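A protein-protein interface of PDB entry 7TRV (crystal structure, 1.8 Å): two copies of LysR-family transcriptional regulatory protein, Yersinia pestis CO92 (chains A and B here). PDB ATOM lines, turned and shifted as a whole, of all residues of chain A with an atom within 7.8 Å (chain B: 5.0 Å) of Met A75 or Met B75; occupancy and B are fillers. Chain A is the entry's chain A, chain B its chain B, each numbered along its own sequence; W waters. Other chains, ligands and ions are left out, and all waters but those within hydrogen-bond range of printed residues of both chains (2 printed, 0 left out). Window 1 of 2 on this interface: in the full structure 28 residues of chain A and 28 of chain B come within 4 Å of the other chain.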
ATOM      1  N   ALA A   3     -13.148   5.487 -10.346  1.00  0.00           N
ATOM      2  CA  ALA A   3     -13.525   5.340 -11.745  1.00  0.00           C
ATOM      3  C   ALA A   3     -15.022   5.144 -11.935  1.00  0.00           C
ATOM      4  O   ALA A   3     -15.501   5.247 -13.070  1.00  0.00           O
ATOM      5  CB  ALA A   3     -12.774   4.163 -12.365  1.00  0.00           C
ATOM      6  N   MET A   4     -15.762   4.867 -10.867  1.00  0.00           N
ATOM      7  CA  MET A   4     -17.182   4.553 -10.966  1.00  0.00           C
ATOM      8  C   MET A   4     -18.080   5.684 -10.474  1.00  0.00           C
ATOM      9  O   MET A   4     -19.228   5.441 -10.102  1.00  0.00           O
ATOM     10  CB  MET A   4     -17.493   3.281 -10.174  1.00  0.00           C
ATOM     11  CG  MET A   4     -16.712   2.057 -10.616  1.00  0.00           C
ATOM     12  SD  MET A   4     -17.123   1.528 -12.447  1.00  0.00           S
ATOM     13  CE  MET A   4     -15.415   1.930 -13.269  1.00  0.00           C
ATOM     14  N   ASP A   6     -19.506   8.345 -12.060  1.00  0.00           N
ATOM     15  CA  ASP A   6     -20.672   8.508 -12.925  1.00  0.00           C
ATOM     16  C   ASP A   6     -20.230   8.178 -14.342  1.00  0.00           C
ATOM     17  O   ASP A   6     -19.466   8.939 -14.943  1.00  0.00           O
ATOM     18  CB  ASP A   6     -21.234   9.923 -12.835  1.00  0.00           C
ATOM     19  CG  ASP A   6     -22.575  10.067 -13.535  1.00  0.00           C
ATOM     20  OD1 ASP A   6     -22.877   9.251 -14.431  1.00  0.00           O
ATOM     21  OD2 ASP A   6     -23.330  11.000 -13.189  1.00  0.00           O
ATOM     22  N   LEU A   7     -20.714   7.054 -14.871  1.00  0.00           N
ATOM     23  CA  LEU A   7     -20.309   6.631 -16.205  1.00  0.00           C
ATOM     24  C   LEU A   7     -20.894   7.512 -17.295  1.00  0.00           C
ATOM     25  O   LEU A   7     -20.337   7.562 -18.396  1.00  0.00           O
ATOM     26  CB  LEU A   7     -20.714   5.179 -16.440  1.00  0.00           C
ATOM     27  CG  LEU A   7     -20.126   4.208 -15.420  1.00  0.00           C
ATOM     28  CD1 LEU A   7     -20.555   2.790 -15.737  1.00  0.00           C
ATOM     29  CD2 LEU A   7     -18.606   4.340 -15.385  1.00  0.00           C
ATOM     30  N   ASN A   8     -22.001   8.204 -17.018  1.00  0.00           N
ATOM     31  CA  ASN A   8     -22.578   9.094 -18.017  1.00  0.00           C
ATOM     32  C   ASN A   8     -21.647  10.253 -18.341  1.00  0.00           C
ATOM     33  O   ASN A   8     -21.633  10.734 -19.480  1.00  0.00           O
ATOM     34  CB  ASN A   8     -23.934   9.606 -17.534  1.00  0.00           C
ATOM     35  CG  ASN A   8     -24.945   8.492 -17.369  1.00  0.00           C
ATOM     36  OD1 ASN A   8     -25.023   7.586 -18.199  1.00  0.00           O
ATOM     37  ND2 ASN A   8     -25.720   8.546 -16.292  1.00  0.00           N
ATOM     38  N   ASP A   9     -20.859  10.710 -17.363  1.00  0.00           N
ATOM     39  CA  ASP A   9     -19.885  11.766 -17.626  1.00  0.00           C
ATOM     40  C   ASP A   9     -18.919  11.362 -18.732  1.00  0.00           C
ATOM     41  O   ASP A   9     -18.598  12.171 -19.611  1.00  0.00           O
ATOM     42  CB  ASP A   9     -19.116  12.108 -16.350  1.00  0.00           C
ATOM     43  CG  ASP A   9     -19.958  12.867 -15.343  1.00  0.00           C
ATOM     44  OD1 ASP A   9     -21.070  13.313 -15.703  1.00  0.00           O
ATOM     45  OD2 ASP A   9     -19.506  13.016 -14.187  1.00  0.00           O
ATOM     46  N   LEU A  10     -18.442  10.117 -18.708  1.00  0.00           N
ATOM     47  CA  LEU A  10     -17.560   9.650 -19.773  1.00  0.00           C
ATOM     48  C   LEU A  10     -18.294   9.580 -21.104  1.00  0.00           C
ATOM     49  O   LEU A  10     -17.706   9.840 -22.160  1.00  0.00           O
ATOM     50  CB  LEU A  10     -16.974   8.286 -19.415  1.00  0.00           C
ATOM     51  CG  LEU A  10     -15.764   8.256 -18.481  1.00  0.00           C
ATOM     52  CD1 LEU A  10     -16.153   8.588 -17.048  1.00  0.00           C
ATOM     53  CD2 LEU A  10     -15.078   6.901 -18.556  1.00  0.00           C
ATOM     54  N   TYR A  11     -19.580   9.231 -21.069  1.00  0.00           N
ATOM     55  CA  TYR A  11     -20.379   9.198 -22.287  1.00  0.00           C
ATOM     56  C   TYR A  11     -20.515  10.593 -22.887  1.00  0.00           C
ATOM     57  O   TYR A  11     -20.276  10.794 -24.084  1.00  0.00           O
ATOM     58  CB  TYR A  11     -21.751   8.596 -21.978  1.00  0.00           C
ATOM     59  CG  TYR A  11     -22.705   8.522 -23.149  1.00  0.00           C
ATOM     60  CD1 TYR A  11     -22.294   8.021 -24.375  1.00  0.00           C
ATOM     61  CD2 TYR A  11     -24.028   8.928 -23.015  1.00  0.00           C
ATOM     62  CE1 TYR A  11     -23.167   7.944 -25.444  1.00  0.00           C
ATOM     63  CE2 TYR A  11     -24.909   8.852 -24.075  1.00  0.00           C
ATOM     64  CZ  TYR A  11     -24.473   8.359 -25.287  1.00  0.00           C
ATOM     65  OH  TYR A  11     -25.345   8.281 -26.345  1.00  0.00           O
ATOM     66  N   TYR A  12     -20.881  11.574 -22.058  1.00  0.00           N
ATOM     67  CA  TYR A  12     -21.091  12.931 -22.555  1.00  0.00           C
ATOM     68  C   TYR A  12     -19.803  13.522 -23.114  1.00  0.00           C
ATOM     69  O   TYR A  12     -19.807  14.138 -24.185  1.00  0.00           O
ATOM     70  CB  TYR A  12     -21.642  13.823 -21.441  1.00  0.00           C
ATOM     71  CG  TYR A  12     -22.938  13.339 -20.822  1.00  0.00           C
ATOM     72  CD1 TYR A  12     -23.797  12.499 -21.518  1.00  0.00           C
ATOM     73  CD2 TYR A  12     -23.302  13.730 -19.539  1.00  0.00           C
ATOM     74  CE1 TYR A  12     -24.978  12.058 -20.954  1.00  0.00           C
ATOM     75  CE2 TYR A  12     -24.477  13.296 -18.969  1.00  0.00           C
ATOM     76  CZ  TYR A  12     -25.316  12.461 -19.678  1.00  0.00           C
ATOM     77  OH  TYR A  12     -26.492  12.026 -19.108  1.00  0.00           O
ATOM     78  N   ALA A  14     -17.139  12.004 -24.394  1.00  0.00           N
ATOM     79  CA  ALA A  14     -16.801  11.402 -25.679  1.00  0.00           C
ATOM     80  C   ALA A  14     -17.744  11.862 -26.781  1.00  0.00           C
ATOM     81  O   ALA A  14     -17.337  11.958 -27.945  1.00  0.00           O
ATOM     82  CB  ALA A  14     -16.820   9.880 -25.570  1.00  0.00           C
ATOM     83  N   TYR A  69     -10.225  10.585 -24.013  1.00  0.00           N
ATOM     84  CA  TYR A  69     -11.363  10.360 -24.899  1.00  0.00           C
ATOM     85  C   TYR A  69     -11.313   8.971 -25.521  1.00  0.00           C
ATOM     86  O   TYR A  69     -12.329   8.271 -25.586  1.00  0.00           O
ATOM     87  CB  TYR A  69     -11.409  11.426 -25.993  1.00  0.00           C
ATOM     88  CG  TYR A  69     -12.147  10.965 -27.234  1.00  0.00           C
ATOM     89  CD1 TYR A  69     -13.535  10.920 -27.264  1.00  0.00           C
ATOM     90  CD2 TYR A  69     -11.454  10.567 -28.371  1.00  0.00           C
ATOM     91  CE1 TYR A  69     -14.212  10.492 -28.390  1.00  0.00           C
ATOM     92  CE2 TYR A  69     -12.124  10.138 -29.503  1.00  0.00           C
ATOM     93  CZ  TYR A  69     -13.503  10.103 -29.507  1.00  0.00           C
ATOM     94  OH  TYR A  69     -14.174   9.677 -30.632  1.00  0.00           O
ATOM     95  N   GLU A  70     -10.138   8.563 -26.005  1.00  0.00           N
ATOM     96  CA  GLU A  70     -10.024   7.258 -26.648  1.00  0.00           C
ATOM     97  C   GLU A  70     -10.402   6.139 -25.684  1.00  0.00           C
ATOM     98  O   GLU A  70     -11.035   5.154 -26.082  1.00  0.00           O
ATOM     99  CB  GLU A  70      -8.609   7.068 -27.191  1.00  0.00           C
ATOM    100  CG  GLU A  70      -8.248   8.060 -28.288  1.00  0.00           C
ATOM    101  CD  GLU A  70      -6.761   8.102 -28.575  1.00  0.00           C
ATOM    102  OE1 GLU A  70      -6.022   7.266 -28.011  1.00  0.00           O
ATOM    103  OE2 GLU A  70      -6.327   8.975 -29.359  1.00  0.00           O
ATOM    104  N   HIS A  71     -10.039   6.285 -24.408  1.00  0.00           N
ATOM    105  CA  HIS A  71     -10.509   5.348 -23.394  1.00  0.00           C
ATOM    106  C   HIS A  71     -12.020   5.431 -23.231  1.00  0.00           C
ATOM    107  O   HIS A  71     -12.694   4.404 -23.081  1.00  0.00           O
ATOM    108  CB  HIS A  71      -9.817   5.624 -22.060  1.00  0.00           C
ATOM    109  CG  HIS A  71      -8.416   5.107 -21.985  1.00  0.00           C
ATOM    110  ND1 HIS A  71      -8.126   3.784 -21.724  1.00  0.00           N
ATOM    111  CD2 HIS A  71      -7.224   5.732 -22.130  1.00  0.00           C
ATOM    112  CE1 HIS A  71      -6.816   3.618 -21.716  1.00  0.00           C
ATOM    113  NE2 HIS A  71      -6.245   4.784 -21.960  1.00  0.00           N
ATOM    114  N   CYS A  72     -12.569   6.648 -23.246  1.00  0.00           N
ATOM    115  CA  CYS A  72     -14.015   6.804 -23.159  1.00  0.00           C
ATOM    116  C   CYS A  72     -14.705   6.153 -24.348  1.00  0.00           C
ATOM    117  O   CYS A  72     -15.760   5.525 -24.200  1.00  0.00           O
ATOM    118  CB  CYS A  72     -14.380   8.285 -23.072  1.00  0.00           C
ATOM    119  SG  CYS A  72     -13.768   9.128 -21.596  1.00  0.00           S
ATOM    120  N   LYS A  73     -14.117   6.287 -25.539  1.00  0.00           N
ATOM    121  CA  LYS A  73     -14.715   5.688 -26.726  1.00  0.00           C
ATOM    122  C   LYS A  73     -14.729   4.169 -26.623  1.00  0.00           C
ATOM    123  O   LYS A  73     -15.676   3.516 -27.076  1.00  0.00           O
ATOM    124  CB  LYS A  73     -13.960   6.138 -27.977  1.00  0.00           C
ATOM    125  CG  LYS A  73     -14.663   5.780 -29.269  1.00  0.00           C
ATOM    126  CD  LYS A  73     -13.993   6.416 -30.476  1.00  0.00           C
ATOM    127  CE  LYS A  73     -12.982   5.479 -31.114  1.00  0.00           C
ATOM    128  NZ  LYS A  73     -12.591   5.953 -32.471  1.00  0.00           N
ATOM    129  N   ALA A  74     -13.689   3.590 -26.022  1.00  0.00           N
ATOM    130  CA  ALA A  74     -13.659   2.144 -25.827  1.00  0.00           C
ATOM    131  C   ALA A  74     -14.798   1.691 -24.921  1.00  0.00           C
ATOM    132  O   ALA A  74     -15.490   0.711 -25.220  1.00  0.00           O
ATOM    133  CB  ALA A  74     -12.310   1.720 -25.249  1.00  0.00           C
ATOM    134  N   MET A  75     -15.006   2.393 -23.809  1.00  0.00           N
ATOM    135  CA  MET A  75     -16.067   2.041 -22.871  1.00  0.00           C
ATOM    136  C   MET A  75     -17.421   2.086 -23.548  1.00  0.00           C
ATOM    137  O   MET A  75     -18.260   1.215 -23.328  1.00  0.00           O
ATOM    138  CB  MET A  75     -16.077   2.976 -21.664  1.00  0.00           C
ATOM    139  CG  MET A  75     -17.194   2.671 -20.682  1.00  0.00           C
ATOM    140  SD  MET A  75     -17.820   4.264 -19.760  1.00  0.00           S
ATOM    141  CE  MET A  75     -18.073   5.411 -21.318  1.00  0.00           C
ATOM    142  N   ILE A  76     -17.624   3.117 -24.371  1.00  0.00           N
ATOM    143  CA  ILE A  76     -18.888   3.266 -25.086  1.00  0.00           C
ATOM    144  C   ILE A  76     -19.108   2.096 -26.032  1.00  0.00           C
ATOM    145  O   ILE A  76     -20.217   1.556 -26.127  1.00  0.00           O
ATOM    146  CB  ILE A  76     -18.924   4.612 -25.831  1.00  0.00           C
ATOM    147  CG1 ILE A  76     -19.046   5.764 -24.837  1.00  0.00           C
ATOM    148  CG2 ILE A  76     -20.066   4.648 -26.844  1.00  0.00           C
ATOM    149  CD1 ILE A  76     -19.151   7.117 -25.497  1.00  0.00           C
ATOM    150  N   GLU A  77     -18.056   1.679 -26.741  1.00  0.00           N
ATOM    151  CA  GLU A  77     -18.195   0.558 -27.663  1.00  0.00           C
ATOM    152  C   GLU A  77     -18.647  -0.701 -26.936  1.00  0.00           C
ATOM    153  O   GLU A  77     -19.453  -1.477 -27.465  1.00  0.00           O
ATOM    154  CB  GLU A  77     -16.876   0.322 -28.395  1.00  0.00           C
ATOM    155  CG  GLU A  77     -16.518   1.438 -29.364  1.00  0.00           C
ATOM    156  CD  GLU A  77     -15.099   1.332 -29.885  1.00  0.00           C
ATOM    157  OE1 GLU A  77     -14.312   0.547 -29.313  1.00  0.00           O
ATOM    158  OE2 GLU A  77     -14.771   2.034 -30.866  1.00  0.00           O
ATOM    159  N   GLU A  78     -18.155  -0.914 -25.714  1.00  0.00           N
ATOM    160  CA  GLU A  78     -18.594  -2.066 -24.934  1.00  0.00           C
ATOM    161  C   GLU A  78     -20.058  -1.937 -24.537  1.00  0.00           C
ATOM    162  O   GLU A  78     -20.823  -2.904 -24.635  1.00  0.00           O
ATOM    163  CB  GLU A  78     -17.718  -2.231 -23.690  1.00  0.00           C
ATOM    164  CG  GLU A  78     -16.237  -2.437 -23.973  1.00  0.00           C
ATOM    165  CD  GLU A  78     -15.934  -3.788 -24.592  1.00  0.00           C
ATOM    166  OE1 GLU A  78     -16.848  -4.632 -24.683  1.00  0.00           O
ATOM    167  OE2 GLU A  78     -14.773  -4.010 -24.991  1.00  0.00           O
ATOM    168  N   ALA A  79     -20.467  -0.750 -24.082  1.00  0.00           N
ATOM    169  CA  ALA A  79     -21.858  -0.550 -23.699  1.00  0.00           C
ATOM    170  C   ALA A  79     -22.797  -0.752 -24.881  1.00  0.00           C
ATOM    171  O   ALA A  79     -23.933  -1.206 -24.700  1.00  0.00           O
ATOM    172  CB  ALA A  79     -22.042   0.843 -23.098  1.00  0.00           C
ATOM    173  N   ARG A  80     -22.348  -0.427 -26.094  1.00  0.00           N
ATOM    174  CA  ARG A  80     -23.175  -0.699 -27.263  1.00  0.00           C
ATOM    175  C   ARG A  80     -23.201  -2.185 -27.588  1.00  0.00           C
ATOM    176  O   ARG A  80     -24.222  -2.697 -28.063  1.00  0.00           O
ATOM    177  CB  ARG A  80     -22.679   0.096 -28.470  1.00  0.00           C
ATOM    178  CG  ARG A  80     -22.837   1.603 -28.344  1.00  0.00           C
ATOM    179  CD  ARG A  80     -22.769   2.261 -29.713  1.00  0.00           C
ATOM    180  NE  ARG A  80     -22.274   3.632 -29.660  1.00  0.00           N
ATOM    181  CZ  ARG A  80     -23.045   4.706 -29.560  1.00  0.00           C
ATOM    182  NH1 ARG A  80     -24.361   4.605 -29.474  1.00  0.00           N
ATOM    183  NH2 ARG A  80     -22.483   5.910 -29.547  1.00  0.00           N
ATOM    184  N   ALA A  81     -22.093  -2.890 -27.349  1.00  0.00           N
ATOM    185  CA  ALA A  81     -22.094  -4.335 -27.543  1.00  0.00           C
ATOM    186  C   ALA A  81     -23.042  -5.020 -26.568  1.00  0.00           C
ATOM    187  O   ALA A  81     -23.653  -6.039 -26.907  1.00  0.00           O
ATOM    188  CB  ALA A  81     -20.675  -4.886 -27.400  1.00  0.00           C
ATOM    189  N   ALA A  82     -23.178  -4.474 -25.357  1.00  0.00           N
ATOM    190  CA  ALA A  82     -24.146  -5.003 -24.404  1.00  0.00           C
ATOM    191  C   ALA A  82     -25.565  -4.846 -24.932  1.00  0.00           C
ATOM    192  O   ALA A  82     -26.356  -5.796 -24.915  1.00  0.00           O
ATOM    193  CB  ALA A  82     -23.986  -4.300 -23.056  1.00  0.00           C
ATOM    194  N   LEU B   7     -25.782   4.655 -18.076  1.00  0.00           N
ATOM    195  CA  LEU B   7     -24.714   3.662 -18.103  1.00  0.00           C
ATOM    196  C   LEU B   7     -24.437   3.070 -16.728  1.00  0.00           C
ATOM    197  O   LEU B   7     -23.914   1.954 -16.642  1.00  0.00           O
ATOM    198  CB  LEU B   7     -23.435   4.276 -18.671  1.00  0.00           C
ATOM    199  CG  LEU B   7     -23.424   4.522 -20.180  1.00  0.00           C
ATOM    200  CD1 LEU B   7     -22.067   5.040 -20.622  1.00  0.00           C
ATOM    201  CD2 LEU B   7     -23.784   3.252 -20.933  1.00  0.00           C
ATOM    202  N   LEU B  10     -25.737  -0.586 -15.994  1.00  0.00           N
ATOM    203  CA  LEU B  10     -24.940  -1.734 -16.413  1.00  0.00           C
ATOM    204  C   LEU B  10     -23.868  -2.059 -15.383  1.00  0.00           C
ATOM    205  O   LEU B  10     -23.495  -3.227 -15.215  1.00  0.00           O
ATOM    206  CB  LEU B  10     -24.310  -1.471 -17.781  1.00  0.00           C
ATOM    207  CG  LEU B  10     -25.206  -1.471 -19.027  1.00  0.00           C
ATOM    208  CD1 LEU B  10     -26.064  -0.216 -19.120  1.00  0.00           C
ATOM    209  CD2 LEU B  10     -24.360  -1.634 -20.283  1.00  0.00           C
ATOM    210  N   TYR B  11     -23.366  -1.038 -14.686  1.00  0.00           N
ATOM    211  CA  TYR B  11     -22.437  -1.263 -13.584  1.00  0.00           C
ATOM    212  C   TYR B  11     -23.157  -1.835 -12.369  1.00  0.00           C
ATOM    213  O   TYR B  11     -22.630  -2.725 -11.689  1.00  0.00           O
ATOM    214  CB  TYR B  11     -21.731   0.048 -13.244  1.00  0.00           C
ATOM    215  CG  TYR B  11     -21.082   0.106 -11.882  1.00  0.00           C
ATOM    216  CD1 TYR B  11     -20.077  -0.783 -11.527  1.00  0.00           C
ATOM    217  CD2 TYR B  11     -21.455   1.077 -10.960  1.00  0.00           C
ATOM    218  CE1 TYR B  11     -19.477  -0.722 -10.285  1.00  0.00           C
ATOM    219  CE2 TYR B  11     -20.858   1.148  -9.719  1.00  0.00           C
ATOM    220  CZ  TYR B  11     -19.870   0.246  -9.387  1.00  0.00           C
ATOM    221  OH  TYR B  11     -19.274   0.316  -8.150  1.00  0.00           O
ATOM    222  N   HIS B  71     -20.616  -8.308 -21.250  1.00  0.00           N
ATOM    223  CA  HIS B  71     -20.300  -7.006 -21.823  1.00  0.00           C
ATOM    224  C   HIS B  71     -20.229  -5.923 -20.754  1.00  0.00           C
ATOM    225  O   HIS B  71     -19.392  -5.017 -20.842  1.00  0.00           O
ATOM    226  CB  HIS B  71     -21.330  -6.639 -22.884  1.00  0.00           C
ATOM    227  CG  HIS B  71     -21.182  -7.401 -24.163  1.00  0.00           C
ATOM    228  ND1 HIS B  71     -19.985  -7.489 -24.841  1.00  0.00           N
ATOM    229  CD2 HIS B  71     -22.083  -8.092 -24.899  1.00  0.00           C
ATOM    230  CE1 HIS B  71     -20.153  -8.210 -25.935  1.00  0.00           C
ATOM    231  NE2 HIS B  71     -21.419  -8.584 -25.997  1.00  0.00           N
ATOM    232  N   CYS B  72     -21.105  -5.988 -19.746  1.00  0.00           N
ATOM    233  CA  CYS B  72     -21.038  -5.028 -18.647  1.00  0.00           C
ATOM    234  C   CYS B  72     -19.701  -5.114 -17.929  1.00  0.00           C
ATOM    235  O   CYS B  72     -19.149  -4.094 -17.501  1.00  0.00           O
ATOM    236  CB  CYS B  72     -22.179  -5.270 -17.659  1.00  0.00           C
ATOM    237  SG  CYS B  72     -23.825  -5.082 -18.346  1.00  0.00           S
ATOM    238  N   LYS B  73     -19.171  -6.329 -17.780  1.00  0.00           N
ATOM    239  CA  LYS B  73     -17.855  -6.500 -17.179  1.00  0.00           C
ATOM    240  C   LYS B  73     -16.783  -5.807 -18.008  1.00  0.00           C
ATOM    241  O   LYS B  73     -15.931  -5.097 -17.463  1.00  0.00           O
ATOM    242  CB  LYS B  73     -17.547  -7.989 -17.031  1.00  0.00           C
ATOM    243  CG  LYS B  73     -16.239  -8.302 -16.333  1.00  0.00           C
ATOM    244  CD  LYS B  73     -15.963  -9.797 -16.378  1.00  0.00           C
ATOM    245  CE  LYS B  73     -14.762 -10.171 -15.533  1.00  0.00           C
ATOM    246  NZ  LYS B  73     -14.406 -11.603 -15.712  1.00  0.00           N
ATOM    247  N   ALA B  74     -16.822  -5.990 -19.331  1.00  0.00           N
ATOM    248  CA  ALA B  74     -15.861  -5.324 -20.203  1.00  0.00           C
ATOM    249  C   ALA B  74     -16.025  -3.809 -20.159  1.00  0.00           C
ATOM    250  O   ALA B  74     -15.036  -3.073 -20.228  1.00  0.00           O
ATOM    251  CB  ALA B  74     -16.009  -5.838 -21.634  1.00  0.00           C
ATOM    252  N   MET B  75     -17.262  -3.329 -20.054  1.00  0.00           N
ATOM    253  CA  MET B  75     -17.527  -1.895 -19.988  1.00  0.00           C
ATOM    254  C   MET B  75     -16.910  -1.288 -18.734  1.00  0.00           C
ATOM    255  O   MET B  75     -16.351  -0.192 -18.773  1.00  0.00           O
ATOM    256  CB  MET B  75     -19.032  -1.614 -20.016  1.00  0.00           C
ATOM    257  CG  MET B  75     -19.379  -0.131 -20.108  1.00  0.00           C
ATOM    258  SD  MET B  75     -21.146   0.359 -19.426  1.00  0.00           S
ATOM    259  CE  MET B  75     -20.925  -0.252 -17.592  1.00  0.00           C
ATOM    260  N   ILE B  76     -17.020  -2.010 -17.617  1.00  0.00           N
ATOM    261  CA  ILE B  76     -16.453  -1.525 -16.364  1.00  0.00           C
ATOM    262  C   ILE B  76     -14.931  -1.492 -16.444  1.00  0.00           C
ATOM    263  O   ILE B  76     -14.287  -0.563 -15.941  1.00  0.00           O
ATOM    264  CB  ILE B  76     -16.940  -2.394 -15.192  1.00  0.00           C
ATOM    265  CG1 ILE B  76     -18.455  -2.272 -15.035  1.00  0.00           C
ATOM    266  CG2 ILE B  76     -16.234  -2.007 -13.901  1.00  0.00           C
ATOM    267  CD1 ILE B  76     -19.023  -3.151 -13.952  1.00  0.00           C
ATOM    268  N   GLU B  77     -14.334  -2.501 -17.079  1.00  0.00           N
ATOM    269  CA  GLU B  77     -12.882  -2.533 -17.213  1.00  0.00           C
ATOM    270  C   GLU B  77     -12.374  -1.346 -18.020  1.00  0.00           C
ATOM    271  O   GLU B  77     -11.361  -0.732 -17.665  1.00  0.00           O
ATOM    272  CB  GLU B  77     -12.450  -3.851 -17.852  1.00  0.00           C
ATOM    273  CG  GLU B  77     -12.792  -5.073 -17.014  1.00  0.00           C
ATOM    274  CD  GLU B  77     -12.346  -6.368 -17.659  1.00  0.00           C
ATOM    275  OE1 GLU B  77     -11.773  -6.315 -18.767  1.00  0.00           O
ATOM    276  OE2 GLU B  77     -12.566  -7.439 -17.056  1.00  0.00           O
ATOM    277  N   GLU B  78     -13.067  -1.005 -19.109  1.00  0.00           N
ATOM    278  CA  GLU B  78     -12.653   0.145 -19.904  1.00  0.00           C
ATOM    279  C   GLU B  78     -12.876   1.449 -19.153  1.00  0.00           C
ATOM    280  O   GLU B  78     -12.100   2.398 -19.316  1.00  0.00           O
ATOM    281  CB  GLU B  78     -13.393   0.155 -21.240  1.00  0.00           C
ATOM    282  CG  GLU B  78     -12.989  -0.974 -22.178  1.00  0.00           C
ATOM    283  CD  GLU B  78     -11.495  -0.985 -22.475  1.00  0.00           C
ATOM    284  OE1 GLU B  78     -10.880   0.102 -22.530  1.00  0.00           O
ATOM    285  OE2 GLU B  78     -10.930  -2.084 -22.650  1.00  0.00           O
ATOM    286  N   ALA B  79     -13.922   1.522 -18.332  1.00  0.00           N
ATOM    287  CA  ALA B  79     -14.098   2.698 -17.490  1.00  0.00           C
ATOM    288  C   ALA B  79     -12.969   2.806 -16.472  1.00  0.00           C
ATOM    289  O   ALA B  79     -12.485   3.907 -16.187  1.00  0.00           O
ATOM    290  CB  ALA B  79     -15.456   2.652 -16.793  1.00  0.00           C
HETATM  291  O   HOH W   1     -10.186   2.481 -21.609  1.00  0.00           O
HETATM  292  O   HOH W   2     -14.152   5.633 -15.205  1.00  0.00           O
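OD1 of Asn A8 sits at hydrogen-bond distance from N of Leu B7, 3.0 Å away.
The side-chain carboxylate (OD1) of Asp A6 lies within hydrogen-bond range of the backbone NH (N) of Asn A8. The side-chain sulfur (SG) of Cys B72 lies close to the backbone carbonyl oxygen (O) of Leu B10 (3.7 Å).
Among the printed residues, pairs that only touch across the chains: Ala A81 with His B71 (3.3 Å), Glu A78 with Ala B74 (3.4 Å), Ala A74 with Glu B78 (3.5 Å), Met A75 with Met B75 (3.5 Å), Ala A82 with His B71 (3.5 Å), Leu A7 with Leu B7 (3.6 Å), Leu A7 with Met B75 (3.6 Å), Met A4 with Ala B79 (3.6 Å), Met A75 with Glu B78 (3.7 Å), Ala A79 with Leu B7 (3.7 Å), Glu A78 with Met B75 (3.7 Å), Ala A79 with Met B75 (3.8 Å), Tyr A11 with Leu B7 (3.8 Å), Met A4 with Ile B76 (3.8 Å), Leu A7 with Ala B79 (3.8 Å), Ala A3 with Ala B79 (3.8 Å), Met A4 with Tyr B11 (3.8 Å), Ala A82 with Leu B10 (3.9 Å), Leu A7 with Tyr B11 (3.9 Å) and Glu A78 with Glu B78 (3.99 Å).
Printed residues of chain B within 4 Å of Leu A7: Leu B7 (3.6 Å), Tyr B11 (3.9 Å), Met B75 (3.6 Å) and Ala B79 (3.8 Å). Tyr A12 touches none of the printed residues of chain B. Printed residues of chain B within 4 Å of Met A75: Met B75 (3.5 Å) and Glu B78 (3.7 Å). Printed residues of chain B within 4 Å of Ala A79: Leu B7 and Met B75. Printed residues of chain B within 4 Å of Ala A82: Leu B10 (3.9 Å) and His B71 (3.5 Å). Of the printed residues of chain A, Leu B10 touches Ala A82. Printed residues of chain A within 4 Å of Tyr B11: Met A4 and Leu A7. Ala B74 touches just one residue of chain A: Glu A78 (3.4 Å). Of the printed residues of chain A, Met B75 touches Leu A7 (3.6 Å), Met A75 (3.5 Å), Glu A78 (3.7 Å) and Ala A79 (3.8 Å). The nearest printed residue of chain A that does not touch Met B75 is Ile A76 (5.6 Å).
Of the 24 printed residues of chain A, 11 touch a printed residue of chain B. Of the 12 printed residues of chain B, 9 touch a printed residue of chain A. Hydrophobic or aromatic side chains of chain B within 4 Å of the printed part of chain A: Leu B7, Leu B10, Tyr B11, His B71, Ala B74, Met B75, Ile B76 and Ala B79. Among the printed residues, no Asp or Glu carboxylate lies within 4 Å of a Lys or Arg side-chain nitrogen of the other chain.
Leu B7 touches its own counterpart, Leu A7. Leu A7 touches Tyr B11, and with the chains exchanged Tyr A11 touches Leu B7. Glu B78 touches its own counterpart, Glu A78. Ala A79 touches Met B75, but with the chains exchanged Met A75 does not touch Ala B79 (4.1 Å). Of the 21 pairs that touch across the chains among the printed residues, 11 have their exchanged pair printed and touching as well.
Water W1 lies within hydrogen-bond range of a ring nitrogen (ND1) of His A71 and the side-chain carboxylate (OE1) of Glu B78. Water W2 bridges O of Ala A3 and O of Ala B79.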
